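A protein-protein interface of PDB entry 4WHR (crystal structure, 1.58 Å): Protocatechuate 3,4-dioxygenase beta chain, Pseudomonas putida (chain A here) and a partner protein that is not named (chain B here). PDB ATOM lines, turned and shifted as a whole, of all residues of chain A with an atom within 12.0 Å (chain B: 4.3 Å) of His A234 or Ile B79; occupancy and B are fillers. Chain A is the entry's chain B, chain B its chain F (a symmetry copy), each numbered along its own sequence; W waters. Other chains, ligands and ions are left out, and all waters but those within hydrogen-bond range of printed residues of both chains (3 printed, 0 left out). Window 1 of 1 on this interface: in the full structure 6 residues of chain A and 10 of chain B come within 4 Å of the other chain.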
ATOM      1  N   ASP A   4     -25.978  11.908  37.796  1.00  0.00           N
ATOM      2  CA  ASP A   4     -25.225  11.271  36.718  1.00  0.00           C
ATOM      3  C   ASP A   4     -25.214   9.764  36.944  1.00  0.00           C
ATOM      4  O   ASP A   4     -24.339   9.236  37.619  1.00  0.00           O
ATOM      5  CB  ASP A   4     -23.791  11.785  36.724  1.00  0.00           C
ATOM      6  CG  ASP A   4     -22.959  11.249  35.585  1.00  0.00           C
ATOM      7  OD1 ASP A   4     -23.440  11.264  34.446  1.00  0.00           O
ATOM      8  OD2 ASP A   4     -21.803  10.821  35.821  1.00  0.00           O
ATOM      9  N   ASN A   5     -26.190   9.072  36.384  1.00  0.00           N
ATOM     10  CA  ASN A   5     -26.230   7.608  36.521  1.00  0.00           C
ATOM     11  C   ASN A   5     -26.356   6.878  35.189  1.00  0.00           C
ATOM     12  O   ASN A   5     -26.374   5.640  35.139  1.00  0.00           O
ATOM     13  CB  ASN A   5     -27.335   7.186  37.489  1.00  0.00           C
ATOM     14  CG  ASN A   5     -28.663   7.848  37.188  1.00  0.00           C
ATOM     15  OD1 ASN A   5     -29.045   8.000  36.027  1.00  0.00           O
ATOM     16  ND2 ASN A   5     -29.380   8.242  38.237  1.00  0.00           N
ATOM     17  N   SER A   6     -26.406   7.628  34.100  1.00  0.00           N
ATOM     18  CA  SER A   6     -26.507   7.005  32.798  1.00  0.00           C
ATOM     19  C   SER A   6     -25.548   7.603  31.791  1.00  0.00           C
ATOM     20  O   SER A   6     -24.953   8.674  32.006  1.00  0.00           O
ATOM     21  CB  SER A   6     -27.933   7.082  32.266  1.00  0.00           C
ATOM     22  OG  SER A   6     -28.264   8.412  31.957  1.00  0.00           O
ATOM     23  N   ARG A   7     -25.389   6.844  30.724  1.00  0.00           N
ATOM     24  CA  ARG A   7     -24.576   7.197  29.576  1.00  0.00           C
ATOM     25  C   ARG A   7     -25.389   7.051  28.307  1.00  0.00           C
ATOM     26  O   ARG A   7     -26.303   6.224  28.214  1.00  0.00           O
ATOM     27  CB  ARG A   7     -23.340   6.298  29.504  1.00  0.00           C
ATOM     28  CG  ARG A   7     -22.402   6.428  30.690  1.00  0.00           C
ATOM     29  CD  ARG A   7     -21.634   7.739  30.631  1.00  0.00           C
ATOM     30  NE  ARG A   7     -20.824   7.978  31.822  1.00  0.00           N
ATOM     31  CZ  ARG A   7     -21.186   8.742  32.854  1.00  0.00           C
ATOM     32  NH1 ARG A   7     -22.371   9.335  32.876  1.00  0.00           N
ATOM     33  NH2 ARG A   7     -20.363   8.906  33.879  1.00  0.00           N
ATOM     34  N   PHE A   8     -25.065   7.873  27.319  1.00  0.00           N
ATOM     35  CA  PHE A   8     -25.764   7.896  26.067  1.00  0.00           C
ATOM     36  C   PHE A   8     -24.851   7.496  24.920  1.00  0.00           C
ATOM     37  O   PHE A   8     -23.741   7.979  24.798  1.00  0.00           O
ATOM     38  CB  PHE A   8     -26.400   9.263  25.840  1.00  0.00           C
ATOM     39  CG  PHE A   8     -27.446   9.577  26.859  1.00  0.00           C
ATOM     40  CD1 PHE A   8     -27.115  10.191  28.052  1.00  0.00           C
ATOM     41  CD2 PHE A   8     -28.764   9.185  26.646  1.00  0.00           C
ATOM     42  CE1 PHE A   8     -28.094  10.436  29.020  1.00  0.00           C
ATOM     43  CE2 PHE A   8     -29.743   9.409  27.595  1.00  0.00           C
ATOM     44  CZ  PHE A   8     -29.420  10.043  28.781  1.00  0.00           C
ATOM     45  N   VAL A   9     -25.345   6.591  24.100  1.00  0.00           N
ATOM     46  CA  VAL A   9     -24.594   6.061  22.987  1.00  0.00           C
ATOM     47  C   VAL A   9     -24.092   7.217  22.136  1.00  0.00           C
ATOM     48  O   VAL A   9     -24.844   8.147  21.826  1.00  0.00           O
ATOM     49  CB  VAL A   9     -25.468   5.109  22.151  1.00  0.00           C
ATOM     50  CG1 VAL A   9     -24.724   4.670  20.891  1.00  0.00           C
ATOM     51  CG2 VAL A   9     -25.837   3.905  23.000  1.00  0.00           C
ATOM     52  N   ILE A  10     -22.812   7.156  21.774  1.00  0.00           N
ATOM     53  CA  ILE A  10     -22.201   8.211  20.965  1.00  0.00           C
ATOM     54  C   ILE A  10     -22.895   8.376  19.610  1.00  0.00           C
ATOM     55  O   ILE A  10     -23.258   7.407  18.939  1.00  0.00           O
ATOM     56  CB  ILE A  10     -20.687   7.954  20.798  1.00  0.00           C
ATOM     57  CG1 ILE A  10     -20.012   7.923  22.171  1.00  0.00           C
ATOM     58  CG2 ILE A  10     -20.063   8.969  19.842  1.00  0.00           C
ATOM     59  CD1 ILE A  10     -20.346   9.087  23.087  1.00  0.00           C
ATOM     60  N   GLN A  41     -18.732  12.199  28.931  1.00  0.00           N
ATOM     61  CA  GLN A  41     -19.991  12.556  29.556  1.00  0.00           C
ATOM     62  C   GLN A  41     -19.786  12.817  31.053  1.00  0.00           C
ATOM     63  O   GLN A  41     -19.072  12.089  31.749  1.00  0.00           O
ATOM     64  CB  GLN A  41     -21.066  11.495  29.295  1.00  0.00           C
ATOM     65  CG  GLN A  41     -21.549  11.558  27.854  1.00  0.00           C
ATOM     66  CD  GLN A  41     -22.416  10.405  27.408  1.00  0.00           C
ATOM     67  OE1 GLN A  41     -23.014   9.718  28.219  1.00  0.00           O
ATOM     68  NE2 GLN A  41     -22.508  10.215  26.106  1.00  0.00           N
ATOM     69  N   THR A  46     -25.449  14.523  30.810  1.00  0.00           N
ATOM     70  CA  THR A  46     -26.324  13.361  30.938  1.00  0.00           C
ATOM     71  C   THR A  46     -27.640  13.625  31.682  1.00  0.00           C
ATOM     72  O   THR A  46     -28.427  12.702  31.912  1.00  0.00           O
ATOM     73  CB  THR A  46     -25.592  12.213  31.640  1.00  0.00           C
ATOM     74  OG1 THR A  46     -25.324  12.567  33.001  1.00  0.00           O
ATOM     75  CG2 THR A  46     -24.299  11.903  30.897  1.00  0.00           C
ATOM     76  N   TYR A  88     -32.043   1.388  22.112  1.00  0.00           N
ATOM     77  CA  TYR A  88     -32.237   0.045  22.651  1.00  0.00           C
ATOM     78  C   TYR A  88     -33.689  -0.407  22.556  1.00  0.00           C
ATOM     79  O   TYR A  88     -34.012  -1.518  23.009  1.00  0.00           O
ATOM     80  CB  TYR A  88     -31.790  -0.023  24.109  1.00  0.00           C
ATOM     81  CG  TYR A  88     -30.319   0.258  24.344  1.00  0.00           C
ATOM     82  CD1 TYR A  88     -29.365  -0.712  24.097  1.00  0.00           C
ATOM     83  CD2 TYR A  88     -29.887   1.480  24.867  1.00  0.00           C
ATOM     84  CE1 TYR A  88     -28.018  -0.471  24.325  1.00  0.00           C
ATOM     85  CE2 TYR A  88     -28.543   1.728  25.098  1.00  0.00           C
ATOM     86  CZ  TYR A  88     -27.611   0.758  24.830  1.00  0.00           C
ATOM     87  OH  TYR A  88     -26.273   1.030  25.058  1.00  0.00           O
ATOM     88  N   GLY A 229     -29.424   5.885  22.561  1.00  0.00           N
ATOM     89  CA  GLY A 229     -29.593   4.841  23.561  1.00  0.00           C
ATOM     90  C   GLY A 229     -29.057   5.258  24.902  1.00  0.00           C
ATOM     91  O   GLY A 229     -27.960   5.835  24.998  1.00  0.00           O
ATOM     92  N   GLN A 230     -29.810   4.934  25.952  1.00  0.00           N
ATOM     93  CA  GLN A 230     -29.426   5.208  27.326  1.00  0.00           C
ATOM     94  C   GLN A 230     -29.072   3.924  28.064  1.00  0.00           C
ATOM     95  O   GLN A 230     -29.835   2.957  28.029  1.00  0.00           O
ATOM     96  CB  GLN A 230     -30.569   5.903  28.055  1.00  0.00           C
ATOM     97  CG  GLN A 230     -30.171   6.397  29.434  1.00  0.00           C
ATOM     98  CD  GLN A 230     -31.263   7.197  30.116  1.00  0.00           C
ATOM     99  OE1 GLN A 230     -32.418   7.268  29.649  1.00  0.00           O
ATOM    100  NE2 GLN A 230     -30.914   7.792  31.221  1.00  0.00           N
ATOM    101  N   ARG A 231     -27.911   3.893  28.687  1.00  0.00           N
ATOM    102  CA  ARG A 231     -27.521   2.745  29.535  1.00  0.00           C
ATOM    103  C   ARG A 231     -26.994   3.209  30.898  1.00  0.00           C
ATOM    104  O   ARG A 231     -26.521   4.344  31.058  1.00  0.00           O
ATOM    105  CB  ARG A 231     -26.460   1.886  28.832  1.00  0.00           C
ATOM    106  CG  ARG A 231     -25.069   2.502  28.706  1.00  0.00           C
ATOM    107  CD  ARG A 231     -24.081   1.417  28.268  1.00  0.00           C
ATOM    108  NE  ARG A 231     -22.729   1.872  27.982  1.00  0.00           N
ATOM    109  CZ  ARG A 231     -21.823   2.250  28.883  1.00  0.00           C
ATOM    110  NH1 ARG A 231     -22.122   2.300  30.174  1.00  0.00           N
ATOM    111  NH2 ARG A 231     -20.586   2.589  28.487  1.00  0.00           N
ATOM    112  N   LYS A 232     -27.025   2.308  31.875  1.00  0.00           N
ATOM    113  CA  LYS A 232     -26.399   2.553  33.146  1.00  0.00           C
ATOM    114  C   LYS A 232     -24.884   2.614  32.968  1.00  0.00           C
ATOM    115  O   LYS A 232     -24.316   1.913  32.142  1.00  0.00           O
ATOM    116  CB  LYS A 232     -26.761   1.457  34.168  1.00  0.00           C
ATOM    117  CG  LYS A 232     -28.223   1.449  34.570  1.00  0.00           C
ATOM    118  CD  LYS A 232     -28.490   0.381  35.627  1.00  0.00           C
ATOM    119  CE  LYS A 232     -29.955   0.364  36.035  1.00  0.00           C
ATOM    120  NZ  LYS A 232     -30.198  -0.487  37.235  1.00  0.00           N
ATOM    121  N   THR A 233     -24.237   3.472  33.743  1.00  0.00           N
ATOM    122  CA  THR A 233     -22.788   3.418  33.877  1.00  0.00           C
ATOM    123  C   THR A 233     -22.338   2.037  34.393  1.00  0.00           C
ATOM    124  O   THR A 233     -23.039   1.393  35.191  1.00  0.00           O
ATOM    125  CB  THR A 233     -22.288   4.494  34.855  1.00  0.00           C
ATOM    126  OG1 THR A 233     -22.806   4.226  36.163  1.00  0.00           O
ATOM    127  CG2 THR A 233     -22.720   5.866  34.421  1.00  0.00           C
ATOM    128  N   HIS A 234     -21.168   1.581  33.954  1.00  0.00           N
ATOM    129  CA  HIS A 234     -20.573   0.389  34.510  1.00  0.00           C
ATOM    130  C   HIS A 234     -19.058   0.461  34.525  1.00  0.00           C
ATOM    131  O   HIS A 234     -18.462   1.059  33.630  1.00  0.00           O
ATOM    132  CB  HIS A 234     -21.044  -0.888  33.794  1.00  0.00           C
ATOM    133  CG  HIS A 234     -21.011  -0.847  32.289  1.00  0.00           C
ATOM    134  ND1 HIS A 234     -19.926  -0.420  31.555  1.00  0.00           N
ATOM    135  CD2 HIS A 234     -21.921  -1.279  31.383  1.00  0.00           C
ATOM    136  CE1 HIS A 234     -20.177  -0.566  30.265  1.00  0.00           C
ATOM    137  NE2 HIS A 234     -21.387  -1.070  30.132  1.00  0.00           N
ATOM    138  N   PHE A 235     -18.464  -0.167  35.539  1.00  0.00           N
ATOM    139  CA  PHE A 235     -17.011  -0.289  35.688  1.00  0.00           C
ATOM    140  C   PHE A 235     -16.251   1.035  35.534  1.00  0.00           C
ATOM    141  O   PHE A 235     -15.162   1.070  34.958  1.00  0.00           O
ATOM    142  CB  PHE A 235     -16.470  -1.303  34.684  1.00  0.00           C
ATOM    143  CG  PHE A 235     -17.034  -2.685  34.834  1.00  0.00           C
ATOM    144  CD1 PHE A 235     -16.585  -3.518  35.847  1.00  0.00           C
ATOM    145  CD2 PHE A 235     -17.995  -3.162  33.948  1.00  0.00           C
ATOM    146  CE1 PHE A 235     -17.092  -4.807  35.976  1.00  0.00           C
ATOM    147  CE2 PHE A 235     -18.512  -4.444  34.071  1.00  0.00           C
ATOM    148  CZ  PHE A 235     -18.062  -5.265  35.090  1.00  0.00           C
ATOM    149  N   GLU A 236     -16.817   2.131  36.040  1.00  0.00           N
ATOM    150  CA  GLU A 236     -16.156   3.436  35.941  1.00  0.00           C
ATOM    151  C   GLU A 236     -15.407   3.783  37.232  1.00  0.00           C
ATOM    152  O   GLU A 236     -15.854   3.441  38.324  1.00  0.00           O
ATOM    153  CB  GLU A 236     -17.164   4.542  35.567  1.00  0.00           C
ATOM    154  CG  GLU A 236     -17.557   4.514  34.089  1.00  0.00           C
ATOM    155  CD  GLU A 236     -18.334   5.743  33.630  1.00  0.00           C
ATOM    156  OE1 GLU A 236     -18.367   6.771  34.369  1.00  0.00           O
ATOM    157  OE2 GLU A 236     -18.906   5.681  32.513  1.00  0.00           O
ATOM    158  N   ASN A 237     -14.265   4.458  37.082  1.00  0.00           N
ATOM    159  CA  ASN A 237     -13.409   4.852  38.204  1.00  0.00           C
ATOM    160  C   ASN A 237     -12.848   3.674  38.981  1.00  0.00           C
ATOM    161  O   ASN A 237     -12.642   3.759  40.185  1.00  0.00           O
ATOM    162  CB  ASN A 237     -14.149   5.807  39.151  1.00  0.00           C
ATOM    163  CG  ASN A 237     -14.599   7.069  38.453  1.00  0.00           C
ATOM    164  OD1 ASN A 237     -13.819   7.701  37.744  1.00  0.00           O
ATOM    165  ND2 ASN A 237     -15.856   7.434  38.637  1.00  0.00           N
ATOM    166  N   CYS A 238     -12.599   2.582  38.265  1.00  0.00           N
ATOM    167  CA  CYS A 238     -11.999   1.378  38.838  1.00  0.00           C
ATOM    168  C   CYS A 238     -11.283   0.571  37.758  1.00  0.00           C
ATOM    169  O   CYS A 238     -10.645  -0.442  38.064  1.00  0.00           O
ATOM    170  CB  CYS A 238     -13.073   0.514  39.508  1.00  0.00           C
ATOM    171  SG  CYS A 238     -14.364  -0.098  38.393  1.00  0.00           S
ATOM    172  N   ILE B  78     -11.532  -5.524  28.349  1.00  0.00           N
ATOM    173  CA  ILE B  78     -12.840  -5.721  27.751  1.00  0.00           C
ATOM    174  C   ILE B  78     -13.885  -6.044  28.809  1.00  0.00           C
ATOM    175  O   ILE B  78     -13.607  -6.691  29.833  1.00  0.00           O
ATOM    176  CB  ILE B  78     -12.859  -6.859  26.691  1.00  0.00           C
ATOM    177  CG1 ILE B  78     -12.384  -8.191  27.281  1.00  0.00           C
ATOM    178  CG2 ILE B  78     -12.005  -6.522  25.477  1.00  0.00           C
ATOM    179  CD1 ILE B  78     -12.654  -9.358  26.352  1.00  0.00           C
ATOM    180  N   ILE B  79     -15.096  -5.608  28.519  1.00  0.00           N
ATOM    181  CA  ILE B  79     -16.299  -6.077  29.195  1.00  0.00           C
ATOM    182  C   ILE B  79     -16.908  -7.188  28.352  1.00  0.00           C
ATOM    183  O   ILE B  79     -16.970  -7.080  27.142  1.00  0.00           O
ATOM    184  CB  ILE B  79     -17.300  -4.912  29.354  1.00  0.00           C
ATOM    185  CG1 ILE B  79     -16.729  -3.881  30.340  1.00  0.00           C
ATOM    186  CG2 ILE B  79     -18.676  -5.412  29.771  1.00  0.00           C
ATOM    187  CD1 ILE B  79     -17.415  -2.531  30.270  1.00  0.00           C
ATOM    188  N   VAL B  80     -17.321  -8.277  29.005  1.00  0.00           N
ATOM    189  CA  VAL B  80     -18.037  -9.365  28.347  1.00  0.00           C
ATOM    190  C   VAL B  80     -19.390  -9.445  29.046  1.00  0.00           C
ATOM    191  O   VAL B  80     -19.433  -9.661  30.242  1.00  0.00           O
ATOM    192  CB  VAL B  80     -17.294 -10.710  28.451  1.00  0.00           C
ATOM    193  CG1 VAL B  80     -18.126 -11.814  27.813  1.00  0.00           C
ATOM    194  CG2 VAL B  80     -15.912 -10.629  27.817  1.00  0.00           C
ATOM    195  N   ALA B  81     -20.453  -9.185  28.304  1.00  0.00           N
ATOM    196  CA  ALA B  81     -21.799  -9.034  28.863  1.00  0.00           C
ATOM    197  C   ALA B  81     -22.821  -9.637  27.928  1.00  0.00           C
ATOM    198  O   ALA B  81     -22.599  -9.760  26.721  1.00  0.00           O
ATOM    199  CB  ALA B  81     -22.118  -7.563  29.104  1.00  0.00           C
ATOM    200  N   PHE B 139     -19.068  -9.330  32.966  1.00  0.00           N
ATOM    201  CA  PHE B 139     -17.722  -9.516  33.480  1.00  0.00           C
ATOM    202  C   PHE B 139     -16.827  -8.410  32.921  1.00  0.00           C
ATOM    203  O   PHE B 139     -17.119  -7.860  31.861  1.00  0.00           O
ATOM    204  CB  PHE B 139     -17.145 -10.853  32.992  1.00  0.00           C
ATOM    205  CG  PHE B 139     -17.866 -12.046  33.521  1.00  0.00           C
ATOM    206  CD1 PHE B 139     -17.608 -12.499  34.812  1.00  0.00           C
ATOM    207  CD2 PHE B 139     -18.797 -12.716  32.741  1.00  0.00           C
ATOM    208  CE1 PHE B 139     -18.284 -13.602  35.323  1.00  0.00           C
ATOM    209  CE2 PHE B 139     -19.468 -13.807  33.245  1.00  0.00           C
ATOM    210  CZ  PHE B 139     -19.200 -14.253  34.532  1.00  0.00           C
ATOM    211  N   ASN B 212     -21.427  -0.594  24.530  1.00  0.00           N
ATOM    212  CA  ASN B 212     -21.169  -0.977  25.914  1.00  0.00           C
ATOM    213  C   ASN B 212     -19.715  -0.684  26.343  1.00  0.00           C
ATOM    214  O   ASN B 212     -19.306  -0.943  27.481  1.00  0.00           O
ATOM    215  CB  ASN B 212     -21.488  -2.469  26.076  1.00  0.00           C
ATOM    216  CG  ASN B 212     -22.412  -2.747  27.232  1.00  0.00           C
ATOM    217  OD1 ASN B 212     -23.180  -1.883  27.642  1.00  0.00           O
ATOM    218  ND2 ASN B 212     -22.334  -3.960  27.778  1.00  0.00           N
ATOM    219  N   ASN B 214     -16.446   1.498  27.435  1.00  0.00           N
ATOM    220  CA  ASN B 214     -16.104   2.705  28.191  1.00  0.00           C
ATOM    221  C   ASN B 214     -15.007   3.445  27.443  1.00  0.00           C
ATOM    222  O   ASN B 214     -13.864   2.970  27.385  1.00  0.00           O
ATOM    223  CB  ASN B 214     -15.629   2.385  29.606  1.00  0.00           C
ATOM    224  CG  ASN B 214     -16.752   1.988  30.524  1.00  0.00           C
ATOM    225  OD1 ASN B 214     -17.926   2.142  30.192  1.00  0.00           O
ATOM    226  ND2 ASN B 214     -16.395   1.450  31.687  1.00  0.00           N
ATOM    227  N   CYS B 218     -12.064   0.711  28.085  1.00  0.00           N
ATOM    228  CA  CYS B 218     -12.192  -0.693  27.710  1.00  0.00           C
ATOM    229  C   CYS B 218     -13.204  -0.883  26.616  1.00  0.00           C
ATOM    230  O   CYS B 218     -14.200  -0.140  26.526  1.00  0.00           O
ATOM    231  CB  CYS B 218     -12.587  -1.524  28.920  1.00  0.00           C
ATOM    232  SG  CYS B 218     -14.226  -1.190  29.584  1.00  0.00           S
ATOM    233  N   LEU B 219     -12.948  -1.883  25.771  1.00  0.00           N
ATOM    234  CA  LEU B 219     -13.928  -2.304  24.784  1.00  0.00           C
ATOM    235  C   LEU B 219     -14.958  -3.241  25.414  1.00  0.00           C
ATOM    236  O   LEU B 219     -14.977  -3.422  26.634  1.00  0.00           O
ATOM    237  CB  LEU B 219     -13.231  -2.901  23.545  1.00  0.00           C
ATOM    238  CG  LEU B 219     -12.620  -1.814  22.654  1.00  0.00           C
ATOM    239  CD1 LEU B 219     -11.601  -2.441  21.708  1.00  0.00           C
ATOM    240  CD2 LEU B 219     -13.690  -1.039  21.883  1.00  0.00           C
ATOM    241  N   ALA B 220     -15.857  -3.760  24.600  1.00  0.00           N
ATOM    242  CA  ALA B 220     -16.897  -4.671  25.079  1.00  0.00           C
ATOM    243  C   ALA B 220     -17.315  -5.622  23.983  1.00  0.00           C
ATOM    244  O   ALA B 220     -17.292  -5.287  22.803  1.00  0.00           O
ATOM    245  CB  ALA B 220     -18.112  -3.887  25.552  1.00  0.00           C
ATOM    246  N   TYR B 221     -17.722  -6.803  24.412  1.00  0.00           N
ATOM    247  CA  TYR B 221     -18.228  -7.873  23.572  1.00  0.00           C
ATOM    248  C   TYR B 221     -19.556  -8.352  24.173  1.00  0.00           C
ATOM    249  O   TYR B 221     -19.727  -8.341  25.411  1.00  0.00           O
ATOM    250  CB  TYR B 221     -17.206  -9.024  23.503  1.00  0.00           C
ATOM    251  CG  TYR B 221     -16.103  -8.738  22.510  1.00  0.00           C
ATOM    252  CD1 TYR B 221     -14.993  -7.994  22.877  1.00  0.00           C
ATOM    253  CD2 TYR B 221     -16.226  -9.126  21.179  1.00  0.00           C
ATOM    254  CE1 TYR B 221     -14.007  -7.679  21.949  1.00  0.00           C
ATOM    255  CE2 TYR B 221     -15.255  -8.828  20.256  1.00  0.00           C
ATOM    256  CZ  TYR B 221     -14.155  -8.096  20.639  1.00  0.00           C
ATOM    257  OH  TYR B 221     -13.194  -7.798  19.694  1.00  0.00           O
HETATM  258  O   HOH W   1     -13.644  -0.190  32.961  1.00  0.00           O
HETATM  259  O   HOH W   2     -19.956   3.171  31.818  1.00  0.00           O
HETATM  260  O   HOH W   3     -25.006  -1.233  25.591  1.00  0.00           O
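The side-chain amide nitrogen of Asn B214 is in hydrogen-bond range of the backbone carbonyl oxygen of His A234 (2.9 Å). NE2 of His A234 sits at hydrogen-bond distance from OD1 of Asn B212 (3.2 Å). NH2 of Arg A231 sits at hydrogen-bond distance from OD1 of Asn B214 (3.2 Å).
The backbone carbonyl oxygen (O) of Phe A235 sits close to the side-chain sulfur (SG) of Cys A238, 3.7 Å away. N of Ile B79 is in hydrogen-bond range of O of Leu B219. O of Arg A231 is in hydrogen-bond range of N of Arg A7, at 2.8 Å. O of Ile B79 sits at hydrogen-bond distance from N of Tyr B221, 2.8 Å away. NH1 of Arg A231 sits at hydrogen-bond distance from NE2 of His A234 (3.4 Å).
Among the printed residues, merely in contact across the chains: His A234 with Ile B79 (3.4 Å), Arg A231 with Asn B212 (3.5 Å), Phe A235 with Asn B214 (3.5 Å) and Phe A235 with Ile B79 (3.8 Å).
Gln A230 touches none of the printed residues of chain B. Printed residues of chain B within 4 Å of Arg A231: Asn B212 and Asn B214. His A234 touches just these residues of chain B: Ile B79 (3.4 Å), Asn B212 (2.9 Å) and Asn B214 (2.9 Å). Of the printed residues of chain B, Phe A235 touches Ile B79 (3.8 Å) and Asn B214 (3.5 Å). Cys A238 touches none of the printed residues of chain B. No residue of chain A comes within 4 Å of Ile B78. Of chain A, only His A234 (3.4 Å) and Phe A235 (3.8 Å) come within 4 Å of Ile B79. No residue of chain A comes within 4 Å of Ala B81. Of chain A, only Arg A231 (3.5 Å) and His A234 (2.9 Å) come within 4 Å of Asn B212. Asn B214 touches three residues of chain A. The nearest printed residue of chain B that does not touch Phe A235 is Phe B139 (4.02 Å).
Of the 20 printed residues of chain A, 3 touch a printed residue of chain B. Hydrophobic or aromatic side chains of chain A within 4 Å of the printed part of chain B: His A234 and Phe A235. Among the printed residues, no Asp or Glu carboxylate lies within 4 Å of a Lys or Arg side-chain nitrogen of the other chain.
Water W3 bridges the side-chain hydroxyl of Tyr A88 (2.6 Å) and the side-chain amide oxygen of Asn B212 (2.8 Å). Water W2 lies within hydrogen-bond range of OD1 of Asn B214 (2.8 Å), OE2 of Glu A236 (2.8 Å), NH1 of Arg A231 (2.9 Å) and N of His A234 (2.9 Å). Water W1 lies within hydrogen-bond range of the backbone carbonyl oxygen (O) of Phe A235 (2.8 Å), the side-chain amide nitrogen (ND2) of Asn B214 (3.4 Å) and the side-chain sulfur (SG) of Cys B218 (3.6 Å).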
